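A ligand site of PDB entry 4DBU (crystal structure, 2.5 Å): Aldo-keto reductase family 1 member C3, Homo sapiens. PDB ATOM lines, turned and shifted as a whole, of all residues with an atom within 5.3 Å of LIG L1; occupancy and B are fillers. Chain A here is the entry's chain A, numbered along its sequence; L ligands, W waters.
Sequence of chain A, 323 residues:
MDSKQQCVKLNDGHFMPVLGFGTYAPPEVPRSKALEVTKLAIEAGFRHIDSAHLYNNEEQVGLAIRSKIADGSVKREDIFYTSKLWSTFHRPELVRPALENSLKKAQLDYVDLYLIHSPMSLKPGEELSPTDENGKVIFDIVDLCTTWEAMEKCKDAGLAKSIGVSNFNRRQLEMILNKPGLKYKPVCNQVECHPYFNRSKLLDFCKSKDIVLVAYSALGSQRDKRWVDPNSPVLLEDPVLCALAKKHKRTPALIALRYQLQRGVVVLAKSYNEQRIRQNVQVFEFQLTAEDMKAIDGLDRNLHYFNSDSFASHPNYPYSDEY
O12 of LG2 L2 sits at hydrogen-bond distance from N of Tyr 24. O13 of LG2 L2 sits at hydrogen-bond distance from OH of Tyr 55. A ring nitrogen (NE2) of His 117 is in hydrogen-bond range of an oxygen (O1) of LIG L1. ND2 of Asn 167 is in hydrogen-bond range of O14 of LG2 L2 (3.0 Å). The side-chain hydroxyl (OH) of Tyr 55 is in hydrogen-bond range of an oxygen (O1) of LIG L1, at 2.7 Å.
The side-chain hydroxyl of Tyr 24 lies within hydrogen-bond range of the guanidinium group of Arg 226, at 3.2 Å. N of Met 120 lies within hydrogen-bond range of OG of Ser 118 (3.0 Å). O of His 117 lies within hydrogen-bond range of ND2 of Asn 167 (3.2 Å). The side-chain hydroxyl (OH) of Tyr 55 is in hydrogen-bond range of the side-chain amino group (NZ) of Lys 84, at 2.8 Å. The side-chain hydroxyl (OH) of Tyr 216 lies within hydrogen-bond range of the side-chain amide oxygen (OD1) of Asn 167 (2.7 Å).
The side-chain amide oxygen of Asn 167 sits close to a fluorine (F3) of LIG L1 (2.8 Å). Tyr 24 touches LIG L1. CD2 of Leu 54 touches C4 of LIG L1, at 3.7 Å. CH2 of Trp 86 touches C8 of LIG L1 (3.9 Å). Ser 118 touches LIG L1 (OG to F1, 3.8 Å). CE of Met 120 touches F1 of LIG L1, at 3.0 Å. Tyr 216 touches LIG L1 (OH to F3, 3.5 Å). Trp 227 touches LIG L1. CZ of Phe 306 touches C12 of LIG L1, 3.2 Å away. CG of Pro 318 touches F1 of LIG L1, 3.5 Å away. 12 residues have an atom within 4 Å of LIG L1: Tyr 24, Leu 54, Tyr 55, Trp 86, His 117, Ser 118, Met 120, Asn 167, Tyr 216, Trp 227, Phe 306 and Pro 318. The nearest printed residue that does not touch LIG L1 is Tyr 319 (4.1 Å).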
ATOM      1  N   TYR A  24     -24.738 -20.970  13.556  1.00  0.00           N
ATOM      2  CA  TYR A  24     -24.367 -19.569  13.342  1.00  0.00           C
ATOM      3  C   TYR A  24     -23.164 -19.409  12.416  1.00  0.00           C
ATOM      4  O   TYR A  24     -22.208 -20.184  12.476  1.00  0.00           O
ATOM      5  CB  TYR A  24     -24.119 -18.817  14.641  1.00  0.00           C
ATOM      6  CG  TYR A  24     -23.765 -17.377  14.380  1.00  0.00           C
ATOM      7  CD1 TYR A  24     -24.761 -16.425  14.170  1.00  0.00           C
ATOM      8  CD2 TYR A  24     -22.450 -16.967  14.295  1.00  0.00           C
ATOM      9  CE1 TYR A  24     -24.443 -15.112  13.899  1.00  0.00           C
ATOM     10  CE2 TYR A  24     -22.125 -15.654  14.031  1.00  0.00           C
ATOM     11  CZ  TYR A  24     -23.126 -14.728  13.838  1.00  0.00           C
ATOM     12  OH  TYR A  24     -22.808 -13.415  13.567  1.00  0.00           O
ATOM     13  N   LEU A  54     -31.423 -14.240  15.747  1.00  0.00           N
ATOM     14  CA  LEU A  54     -30.284 -13.375  15.511  1.00  0.00           C
ATOM     15  C   LEU A  54     -29.425 -13.907  14.358  1.00  0.00           C
ATOM     16  O   LEU A  54     -28.850 -13.125  13.596  1.00  0.00           O
ATOM     17  CB  LEU A  54     -29.432 -13.245  16.781  1.00  0.00           C
ATOM     18  CG  LEU A  54     -28.149 -12.425  16.652  1.00  0.00           C
ATOM     19  CD1 LEU A  54     -28.483 -10.966  16.384  1.00  0.00           C
ATOM     20  CD2 LEU A  54     -27.294 -12.560  17.902  1.00  0.00           C
ATOM     21  N   TYR A  55     -29.381 -15.225  14.225  1.00  0.00           N
ATOM     22  CA  TYR A  55     -28.528 -15.866  13.219  1.00  0.00           C
ATOM     23  C   TYR A  55     -28.933 -15.513  11.787  1.00  0.00           C
ATOM     24  O   TYR A  55     -28.098 -15.537  10.886  1.00  0.00           O
ATOM     25  CB  TYR A  55     -28.538 -17.388  13.392  1.00  0.00           C
ATOM     26  CG  TYR A  55     -28.048 -17.857  14.743  1.00  0.00           C
ATOM     27  CD1 TYR A  55     -28.020 -19.206  15.066  1.00  0.00           C
ATOM     28  CD2 TYR A  55     -27.611 -16.956  15.698  1.00  0.00           C
ATOM     29  CE1 TYR A  55     -27.568 -19.642  16.291  1.00  0.00           C
ATOM     30  CE2 TYR A  55     -27.167 -17.373  16.932  1.00  0.00           C
ATOM     31  CZ  TYR A  55     -27.136 -18.722  17.226  1.00  0.00           C
ATOM     32  OH  TYR A  55     -26.699 -19.138  18.453  1.00  0.00           O
ATOM     33  N   LYS A  84     -34.098 -19.011  19.554  1.00  0.00           N
ATOM     34  CA  LYS A  84     -33.888 -18.104  20.673  1.00  0.00           C
ATOM     35  C   LYS A  84     -34.592 -16.753  20.511  1.00  0.00           C
ATOM     36  O   LYS A  84     -34.523 -16.130  19.449  1.00  0.00           O
ATOM     37  CB  LYS A  84     -32.382 -17.890  20.896  1.00  0.00           C
ATOM     38  CG  LYS A  84     -31.551 -19.172  20.932  1.00  0.00           C
ATOM     39  CD  LYS A  84     -30.119 -18.894  21.400  1.00  0.00           C
ATOM     40  CE  LYS A  84     -29.201 -20.070  21.128  1.00  0.00           C
ATOM     41  NZ  LYS A  84     -28.991 -20.295  19.675  1.00  0.00           N
ATOM     42  N   TRP A  86     -34.568 -13.070  20.864  1.00  0.00           N
ATOM     43  CA  TRP A  86     -33.487 -12.095  20.962  1.00  0.00           C
ATOM     44  C   TRP A  86     -33.807 -10.982  21.960  1.00  0.00           C
ATOM     45  O   TRP A  86     -34.964 -10.817  22.380  1.00  0.00           O
ATOM     46  CB  TRP A  86     -33.125 -11.528  19.584  1.00  0.00           C
ATOM     47  CG  TRP A  86     -31.948 -10.604  19.639  1.00  0.00           C
ATOM     48  CD1 TRP A  86     -31.876  -9.328  19.182  1.00  0.00           C
ATOM     49  CD2 TRP A  86     -30.673 -10.899  20.217  1.00  0.00           C
ATOM     50  NE1 TRP A  86     -30.626  -8.806  19.424  1.00  0.00           N
ATOM     51  CE2 TRP A  86     -29.869  -9.750  20.058  1.00  0.00           C
ATOM     52  CE3 TRP A  86     -30.124 -12.023  20.847  1.00  0.00           C
ATOM     53  CZ2 TRP A  86     -28.552  -9.689  20.513  1.00  0.00           C
ATOM     54  CZ3 TRP A  86     -28.808 -11.965  21.289  1.00  0.00           C
ATOM     55  CH2 TRP A  86     -28.036 -10.804  21.121  1.00  0.00           C
ATOM     56  N   HIS A 117     -32.286 -15.762  24.650  1.00  0.00           N
ATOM     57  CA  HIS A 117     -30.937 -15.633  24.109  1.00  0.00           C
ATOM     58  C   HIS A 117     -29.982 -14.975  25.095  1.00  0.00           C
ATOM     59  O   HIS A 117     -28.908 -15.496  25.379  1.00  0.00           O
ATOM     60  CB  HIS A 117     -30.965 -14.838  22.800  1.00  0.00           C
ATOM     61  CG  HIS A 117     -29.817 -15.150  21.884  1.00  0.00           C
ATOM     62  ND1 HIS A 117     -30.010 -15.547  20.575  1.00  0.00           N
ATOM     63  CD2 HIS A 117     -28.483 -15.141  22.080  1.00  0.00           C
ATOM     64  CE1 HIS A 117     -28.834 -15.763  20.005  1.00  0.00           C
ATOM     65  NE2 HIS A 117     -27.892 -15.516  20.899  1.00  0.00           N
ATOM     66  N   SER A 118     -30.378 -13.812  25.629  1.00  0.00           N
ATOM     67  CA  SER A 118     -29.543 -13.068  26.560  1.00  0.00           C
ATOM     68  C   SER A 118     -30.400 -12.318  27.570  1.00  0.00           C
ATOM     69  O   SER A 118     -31.486 -11.863  27.248  1.00  0.00           O
ATOM     70  CB  SER A 118     -28.672 -12.071  25.791  1.00  0.00           C
ATOM     71  OG  SER A 118     -28.102 -11.084  26.643  1.00  0.00           O
ATOM     72  N   PRO A 119     -29.908 -12.196  28.810  1.00  0.00           N
ATOM     73  CA  PRO A 119     -30.630 -11.453  29.857  1.00  0.00           C
ATOM     74  C   PRO A 119     -30.524  -9.950  29.631  1.00  0.00           C
ATOM     75  O   PRO A 119     -31.241  -9.175  30.274  1.00  0.00           O
ATOM     76  CB  PRO A 119     -29.896 -11.845  31.136  1.00  0.00           C
ATOM     77  CG  PRO A 119     -28.522 -12.188  30.681  1.00  0.00           C
ATOM     78  CD  PRO A 119     -28.691 -12.840  29.345  1.00  0.00           C
ATOM     79  N   MET A 120     -29.637  -9.543  28.733  1.00  0.00           N
ATOM     80  CA  MET A 120     -29.391  -8.132  28.473  1.00  0.00           C
ATOM     81  C   MET A 120     -30.416  -7.544  27.511  1.00  0.00           C
ATOM     82  O   MET A 120     -30.232  -7.572  26.288  1.00  0.00           O
ATOM     83  CB  MET A 120     -27.976  -7.907  27.964  1.00  0.00           C
ATOM     84  CG  MET A 120     -26.922  -8.130  29.040  1.00  0.00           C
ATOM     85  SD  MET A 120     -25.250  -7.816  28.477  1.00  0.00           S
ATOM     86  CE  MET A 120     -24.943  -9.246  27.454  1.00  0.00           C
ATOM     87  N   ASN A 167     -26.987 -17.510  28.564  1.00  0.00           N
ATOM     88  CA  ASN A 167     -26.159 -16.422  29.098  1.00  0.00           C
ATOM     89  C   ASN A 167     -26.640 -15.903  30.442  1.00  0.00           C
ATOM     90  O   ASN A 167     -26.373 -14.755  30.798  1.00  0.00           O
ATOM     91  CB  ASN A 167     -26.045 -15.292  28.082  1.00  0.00           C
ATOM     92  CG  ASN A 167     -25.240 -15.682  26.860  1.00  0.00           C
ATOM     93  OD1 ASN A 167     -24.197 -16.327  26.977  1.00  0.00           O
ATOM     94  ND2 ASN A 167     -25.715 -15.289  25.680  1.00  0.00           N
ATOM     95  N   TYR A 216     -21.641 -23.538  24.529  1.00  0.00           N
ATOM     96  CA  TYR A 216     -21.291 -22.989  23.217  1.00  0.00           C
ATOM     97  C   TYR A 216     -19.865 -22.461  23.221  1.00  0.00           C
ATOM     98  O   TYR A 216     -19.315 -22.172  24.286  1.00  0.00           O
ATOM     99  CB  TYR A 216     -22.305 -21.932  22.746  1.00  0.00           C
ATOM    100  CG  TYR A 216     -22.230 -20.586  23.463  1.00  0.00           C
ATOM    101  CD1 TYR A 216     -23.235 -20.178  24.323  1.00  0.00           C
ATOM    102  CD2 TYR A 216     -21.174 -19.712  23.238  1.00  0.00           C
ATOM    103  CE1 TYR A 216     -23.193 -18.948  24.960  1.00  0.00           C
ATOM    104  CE2 TYR A 216     -21.116 -18.484  23.859  1.00  0.00           C
ATOM    105  CZ  TYR A 216     -22.121 -18.108  24.729  1.00  0.00           C
ATOM    106  OH  TYR A 216     -22.063 -16.880  25.351  1.00  0.00           O
ATOM    107  N   ARG A 226     -15.170  -9.010  15.887  1.00  0.00           N
ATOM    108  CA  ARG A 226     -16.116  -8.051  16.437  1.00  0.00           C
ATOM    109  C   ARG A 226     -16.287  -8.186  17.948  1.00  0.00           C
ATOM    110  O   ARG A 226     -16.772  -7.262  18.608  1.00  0.00           O
ATOM    111  CB  ARG A 226     -17.470  -8.181  15.731  1.00  0.00           C
ATOM    112  CG  ARG A 226     -17.419  -7.897  14.242  1.00  0.00           C
ATOM    113  CD  ARG A 226     -18.814  -7.916  13.631  1.00  0.00           C
ATOM    114  NE  ARG A 226     -19.414  -9.245  13.697  1.00  0.00           N
ATOM    115  CZ  ARG A 226     -20.664  -9.518  13.333  1.00  0.00           C
ATOM    116  NH1 ARG A 226     -21.134 -10.749  13.426  1.00  0.00           N
ATOM    117  NH2 ARG A 226     -21.451  -8.541  12.885  1.00  0.00           N
ATOM    118  N   TRP A 227     -15.870  -9.320  18.495  1.00  0.00           N
ATOM    119  CA  TRP A 227     -15.988  -9.555  19.929  1.00  0.00           C
ATOM    120  C   TRP A 227     -14.761 -10.273  20.501  1.00  0.00           C
ATOM    121  O   TRP A 227     -14.447 -10.121  21.678  1.00  0.00           O
ATOM    122  CB  TRP A 227     -17.240 -10.381  20.250  1.00  0.00           C
ATOM    123  CG  TRP A 227     -18.513  -9.768  19.751  1.00  0.00           C
ATOM    124  CD1 TRP A 227     -19.238  -8.780  20.357  1.00  0.00           C
ATOM    125  CD2 TRP A 227     -19.212 -10.110  18.558  1.00  0.00           C
ATOM    126  NE1 TRP A 227     -20.351  -8.483  19.611  1.00  0.00           N
ATOM    127  CE2 TRP A 227     -20.360  -9.277  18.494  1.00  0.00           C
ATOM    128  CE3 TRP A 227     -18.992 -11.021  17.527  1.00  0.00           C
ATOM    129  CZ2 TRP A 227     -21.271  -9.350  17.440  1.00  0.00           C
ATOM    130  CZ3 TRP A 227     -19.892 -11.086  16.477  1.00  0.00           C
ATOM    131  CH2 TRP A 227     -21.018 -10.252  16.448  1.00  0.00           C
ATOM    132  N   PHE A 306     -16.137 -14.311  23.820  1.00  0.00           N
ATOM    133  CA  PHE A 306     -17.066 -13.234  23.492  1.00  0.00           C
ATOM    134  C   PHE A 306     -16.851 -12.069  24.456  1.00  0.00           C
ATOM    135  O   PHE A 306     -17.438 -12.022  25.539  1.00  0.00           O
ATOM    136  CB  PHE A 306     -18.517 -13.710  23.533  1.00  0.00           C
ATOM    137  CG  PHE A 306     -19.451 -12.847  22.752  1.00  0.00           C
ATOM    138  CD1 PHE A 306     -19.873 -13.211  21.486  1.00  0.00           C
ATOM    139  CD2 PHE A 306     -19.902 -11.637  23.276  1.00  0.00           C
ATOM    140  CE1 PHE A 306     -20.725 -12.416  20.758  1.00  0.00           C
ATOM    141  CE2 PHE A 306     -20.769 -10.823  22.551  1.00  0.00           C
ATOM    142  CZ  PHE A 306     -21.174 -11.216  21.292  1.00  0.00           C
ATOM    143  N   PHE A 311     -21.340  -4.393  26.590  1.00  0.00           N
ATOM    144  CA  PHE A 311     -22.411  -4.972  27.407  1.00  0.00           C
ATOM    145  C   PHE A 311     -22.091  -4.946  28.898  1.00  0.00           C
ATOM    146  O   PHE A 311     -22.987  -5.045  29.731  1.00  0.00           O
ATOM    147  CB  PHE A 311     -22.703  -6.405  26.971  1.00  0.00           C
ATOM    148  CG  PHE A 311     -22.986  -6.534  25.502  1.00  0.00           C
ATOM    149  CD1 PHE A 311     -22.375  -7.538  24.754  1.00  0.00           C
ATOM    150  CD2 PHE A 311     -23.854  -5.676  24.867  1.00  0.00           C
ATOM    151  CE1 PHE A 311     -22.626  -7.663  23.407  1.00  0.00           C
ATOM    152  CE2 PHE A 311     -24.107  -5.792  23.511  1.00  0.00           C
ATOM    153  CZ  PHE A 311     -23.496  -6.792  22.776  1.00  0.00           C
ATOM    154  N   TYR A 317     -25.721  -7.768  32.634  1.00  0.00           N
ATOM    155  CA  TYR A 317     -24.486  -8.337  32.104  1.00  0.00           C
ATOM    156  C   TYR A 317     -24.131  -9.598  32.903  1.00  0.00           C
ATOM    157  O   TYR A 317     -23.810  -9.515  34.094  1.00  0.00           O
ATOM    158  CB  TYR A 317     -23.371  -7.285  32.205  1.00  0.00           C
ATOM    159  CG  TYR A 317     -22.004  -7.757  31.769  1.00  0.00           C
ATOM    160  CD1 TYR A 317     -21.742  -8.071  30.437  1.00  0.00           C
ATOM    161  CD2 TYR A 317     -20.962  -7.846  32.678  1.00  0.00           C
ATOM    162  CE1 TYR A 317     -20.491  -8.486  30.036  1.00  0.00           C
ATOM    163  CE2 TYR A 317     -19.704  -8.262  32.285  1.00  0.00           C
ATOM    164  CZ  TYR A 317     -19.475  -8.577  30.970  1.00  0.00           C
ATOM    165  OH  TYR A 317     -18.211  -8.994  30.583  1.00  0.00           O
ATOM    166  N   PRO A 318     -24.197 -10.766  32.241  1.00  0.00           N
ATOM    167  CA  PRO A 318     -24.082 -12.083  32.875  1.00  0.00           C
ATOM    168  C   PRO A 318     -22.861 -12.224  33.787  1.00  0.00           C
ATOM    169  O   PRO A 318     -22.949 -12.911  34.804  1.00  0.00           O
ATOM    170  CB  PRO A 318     -23.940 -13.038  31.678  1.00  0.00           C
ATOM    171  CG  PRO A 318     -23.627 -12.176  30.509  1.00  0.00           C
ATOM    172  CD  PRO A 318     -24.293 -10.880  30.776  1.00  0.00           C
ATOM    173  N   TYR A 319     -21.754 -11.597  33.428  1.00  0.00           N
ATOM    174  CA  TYR A 319     -20.523 -11.723  34.193  1.00  0.00           C
ATOM    175  C   TYR A 319     -20.358 -10.562  35.177  1.00  0.00           C
ATOM    176  O   TYR A 319     -20.807  -9.450  34.922  1.00  0.00           O
ATOM    177  CB  TYR A 319     -19.314 -11.789  33.263  1.00  0.00           C
ATOM    178  CG  TYR A 319     -19.480 -12.745  32.096  1.00  0.00           C
ATOM    179  CD1 TYR A 319     -19.712 -14.099  32.307  1.00  0.00           C
ATOM    180  CD2 TYR A 319     -19.403 -12.296  30.784  1.00  0.00           C
ATOM    181  CE1 TYR A 319     -19.865 -14.977  31.248  1.00  0.00           C
ATOM    182  CE2 TYR A 319     -19.559 -13.164  29.715  1.00  0.00           C
ATOM    183  CZ  TYR A 319     -19.794 -14.505  29.959  1.00  0.00           C
ATOM    184  OH  TYR A 319     -19.943 -15.374  28.898  1.00  0.00           O
HETATM  185  C1  LIG L   1     -23.470 -14.611  17.436  1.00  0.00           C
HETATM  186  C2  LIG L   1     -23.122 -13.255  17.462  1.00  0.00           C
HETATM  187  C3  LIG L   1     -23.401 -12.473  18.575  1.00  0.00           C
HETATM  188  C4  LIG L   1     -24.068 -13.029  19.689  1.00  0.00           C
HETATM  189  C5  LIG L   1     -24.410 -14.389  19.657  1.00  0.00           C
HETATM  190  C6  LIG L   1     -24.126 -15.177  18.538  1.00  0.00           C
HETATM  191  N1  LIG L   1     -24.285 -12.168  20.780  1.00  0.00           N
HETATM  192  C7  LIG L   1     -24.041 -12.321  22.155  1.00  0.00           C
HETATM  193  C8  LIG L   1     -24.744 -11.466  23.016  1.00  0.00           C
HETATM  194  C9  LIG L   1     -24.552 -11.546  24.393  1.00  0.00           C
HETATM  195  C10 LIG L   1     -23.649 -12.460  24.947  1.00  0.00           C
HETATM  196  C11 LIG L   1     -22.952 -13.311  24.092  1.00  0.00           C
HETATM  197  C12 LIG L   1     -23.143 -13.245  22.711  1.00  0.00           C
HETATM  198  C13 LIG L   1     -24.522 -16.613  18.549  1.00  0.00           C
HETATM  199  O1  LIG L   1     -25.377 -16.982  19.366  1.00  0.00           O
HETATM  200  O2  LIG L   1     -23.997 -17.498  17.688  1.00  0.00           O
HETATM  201  C14 LIG L   1     -23.437 -12.549  26.430  1.00  0.00           C
HETATM  202  F1  LIG L   1     -24.508 -12.221  27.134  1.00  0.00           F
HETATM  203  F2  LIG L   1     -22.436 -11.767  26.802  1.00  0.00           F
HETATM  204  F3  LIG L   1     -23.091 -13.789  26.740  1.00  0.00           F
HETATM  205  P1  LG2 L   2     -17.545 -23.270  17.881  1.00  0.00           P
HETATM  206  O1  LG2 L   2     -16.941 -22.565  19.042  1.00  0.00           O
HETATM  207  O2  LG2 L   2     -18.296 -24.583  18.414  1.00  0.00           O
HETATM  208  O3  LG2 L   2     -16.401 -23.727  16.840  1.00  0.00           O
HETATM  209  C1  LG2 L   2     -15.908 -22.550  16.190  1.00  0.00           C
HETATM  210  C2  LG2 L   2     -14.976 -23.005  15.060  1.00  0.00           C
HETATM  211  O4  LG2 L   2     -14.567 -24.355  15.312  1.00  0.00           O
HETATM  212  C3  LG2 L   2     -15.706 -23.036  13.713  1.00  0.00           C
HETATM  213  O5  LG2 L   2     -15.397 -21.868  12.946  1.00  0.00           O
HETATM  214  C4  LG2 L   2     -15.183 -24.319  13.013  1.00  0.00           C
HETATM  215  O6  LG2 L   2     -14.461 -23.993  11.818  1.00  0.00           O
HETATM  216  C5  LG2 L   2     -14.224 -24.954  14.047  1.00  0.00           C
HETATM  217  N1  LG2 L   2     -14.374 -26.405  14.126  1.00  0.00           N
HETATM  218  C6  LG2 L   2     -15.544 -27.091  14.331  1.00  0.00           C
HETATM  219  N2  LG2 L   2     -15.300 -28.374  14.373  1.00  0.00           N
HETATM  220  C7  LG2 L   2     -13.975 -28.594  14.202  1.00  0.00           C
HETATM  221  C8  LG2 L   2     -13.159 -29.734  14.157  1.00  0.00           C
HETATM  222  N3  LG2 L   2     -13.692 -31.008  14.305  1.00  0.00           N
HETATM  223  N4  LG2 L   2     -11.853 -29.577  13.967  1.00  0.00           N
HETATM  224  C9  LG2 L   2     -11.331 -28.378  13.821  1.00  0.00           C
HETATM  225  N5  LG2 L   2     -12.055 -27.276  13.856  1.00  0.00           N
HETATM  226  C10 LG2 L   2     -13.364 -27.337  14.046  1.00  0.00           C
HETATM  227  O7  LG2 L   2     -18.623 -22.328  17.123  1.00  0.00           O
HETATM  228  P2  LG2 L   2     -19.334 -21.298  18.139  1.00  0.00           P
HETATM  229  O8  LG2 L   2     -20.135 -20.256  17.322  1.00  0.00           O
HETATM  230  O9  LG2 L   2     -18.303 -20.543  19.007  1.00  0.00           O
HETATM  231  O10 LG2 L   2     -20.351 -22.109  19.099  1.00  0.00           O
HETATM  232  C11 LG2 L   2     -21.046 -23.055  18.288  1.00  0.00           C
HETATM  233  C12 LG2 L   2     -22.544 -22.784  18.365  1.00  0.00           C
HETATM  234  O11 LG2 L   2     -22.859 -22.252  19.678  1.00  0.00           O
HETATM  235  C13 LG2 L   2     -22.924 -21.653  17.393  1.00  0.00           C
HETATM  236  O12 LG2 L   2     -23.153 -22.163  16.077  1.00  0.00           O
HETATM  237  C14 LG2 L   2     -24.218 -21.110  18.032  1.00  0.00           C
HETATM  238  O13 LG2 L   2     -25.369 -21.820  17.589  1.00  0.00           O
HETATM  239  C15 LG2 L   2     -23.971 -21.319  19.550  1.00  0.00           C
HETATM  240  N6  LG2 L   2     -23.668 -20.034  20.180  1.00  0.00           N
HETATM  241  C16 LG2 L   2     -24.535 -19.497  21.035  1.00  0.00           C
HETATM  242  C17 LG2 L   2     -24.279 -18.269  21.634  1.00  0.00           C
HETATM  243  C18 LG2 L   2     -25.225 -17.667  22.600  1.00  0.00           C
HETATM  244  O14 LG2 L   2     -25.052 -16.530  22.989  1.00  0.00           O
HETATM  245  N7  LG2 L   2     -26.230 -18.402  23.127  1.00  0.00           N
HETATM  246  C19 LG2 L   2     -23.098 -17.593  21.320  1.00  0.00           C
HETATM  247  C20 LG2 L   2     -22.222 -18.184  20.423  1.00  0.00           C
HETATM  248  C21 LG2 L   2     -22.549 -19.409  19.865  1.00  0.00           C
HETATM  249  P3  LG2 L   2     -15.300 -24.516  10.544  1.00  0.00           P
HETATM  250  O15 LG2 L   2     -16.688 -24.024  10.641  1.00  0.00           O
HETATM  251  O16 LG2 L   2     -14.635 -23.931   9.212  1.00  0.00           O
HETATM  252  O17 LG2 L   2     -15.307 -26.135  10.479  1.00  0.00           O
HETATM  253  O   HOH W   1     -24.646  -9.338  19.550  1.00  0.00           O
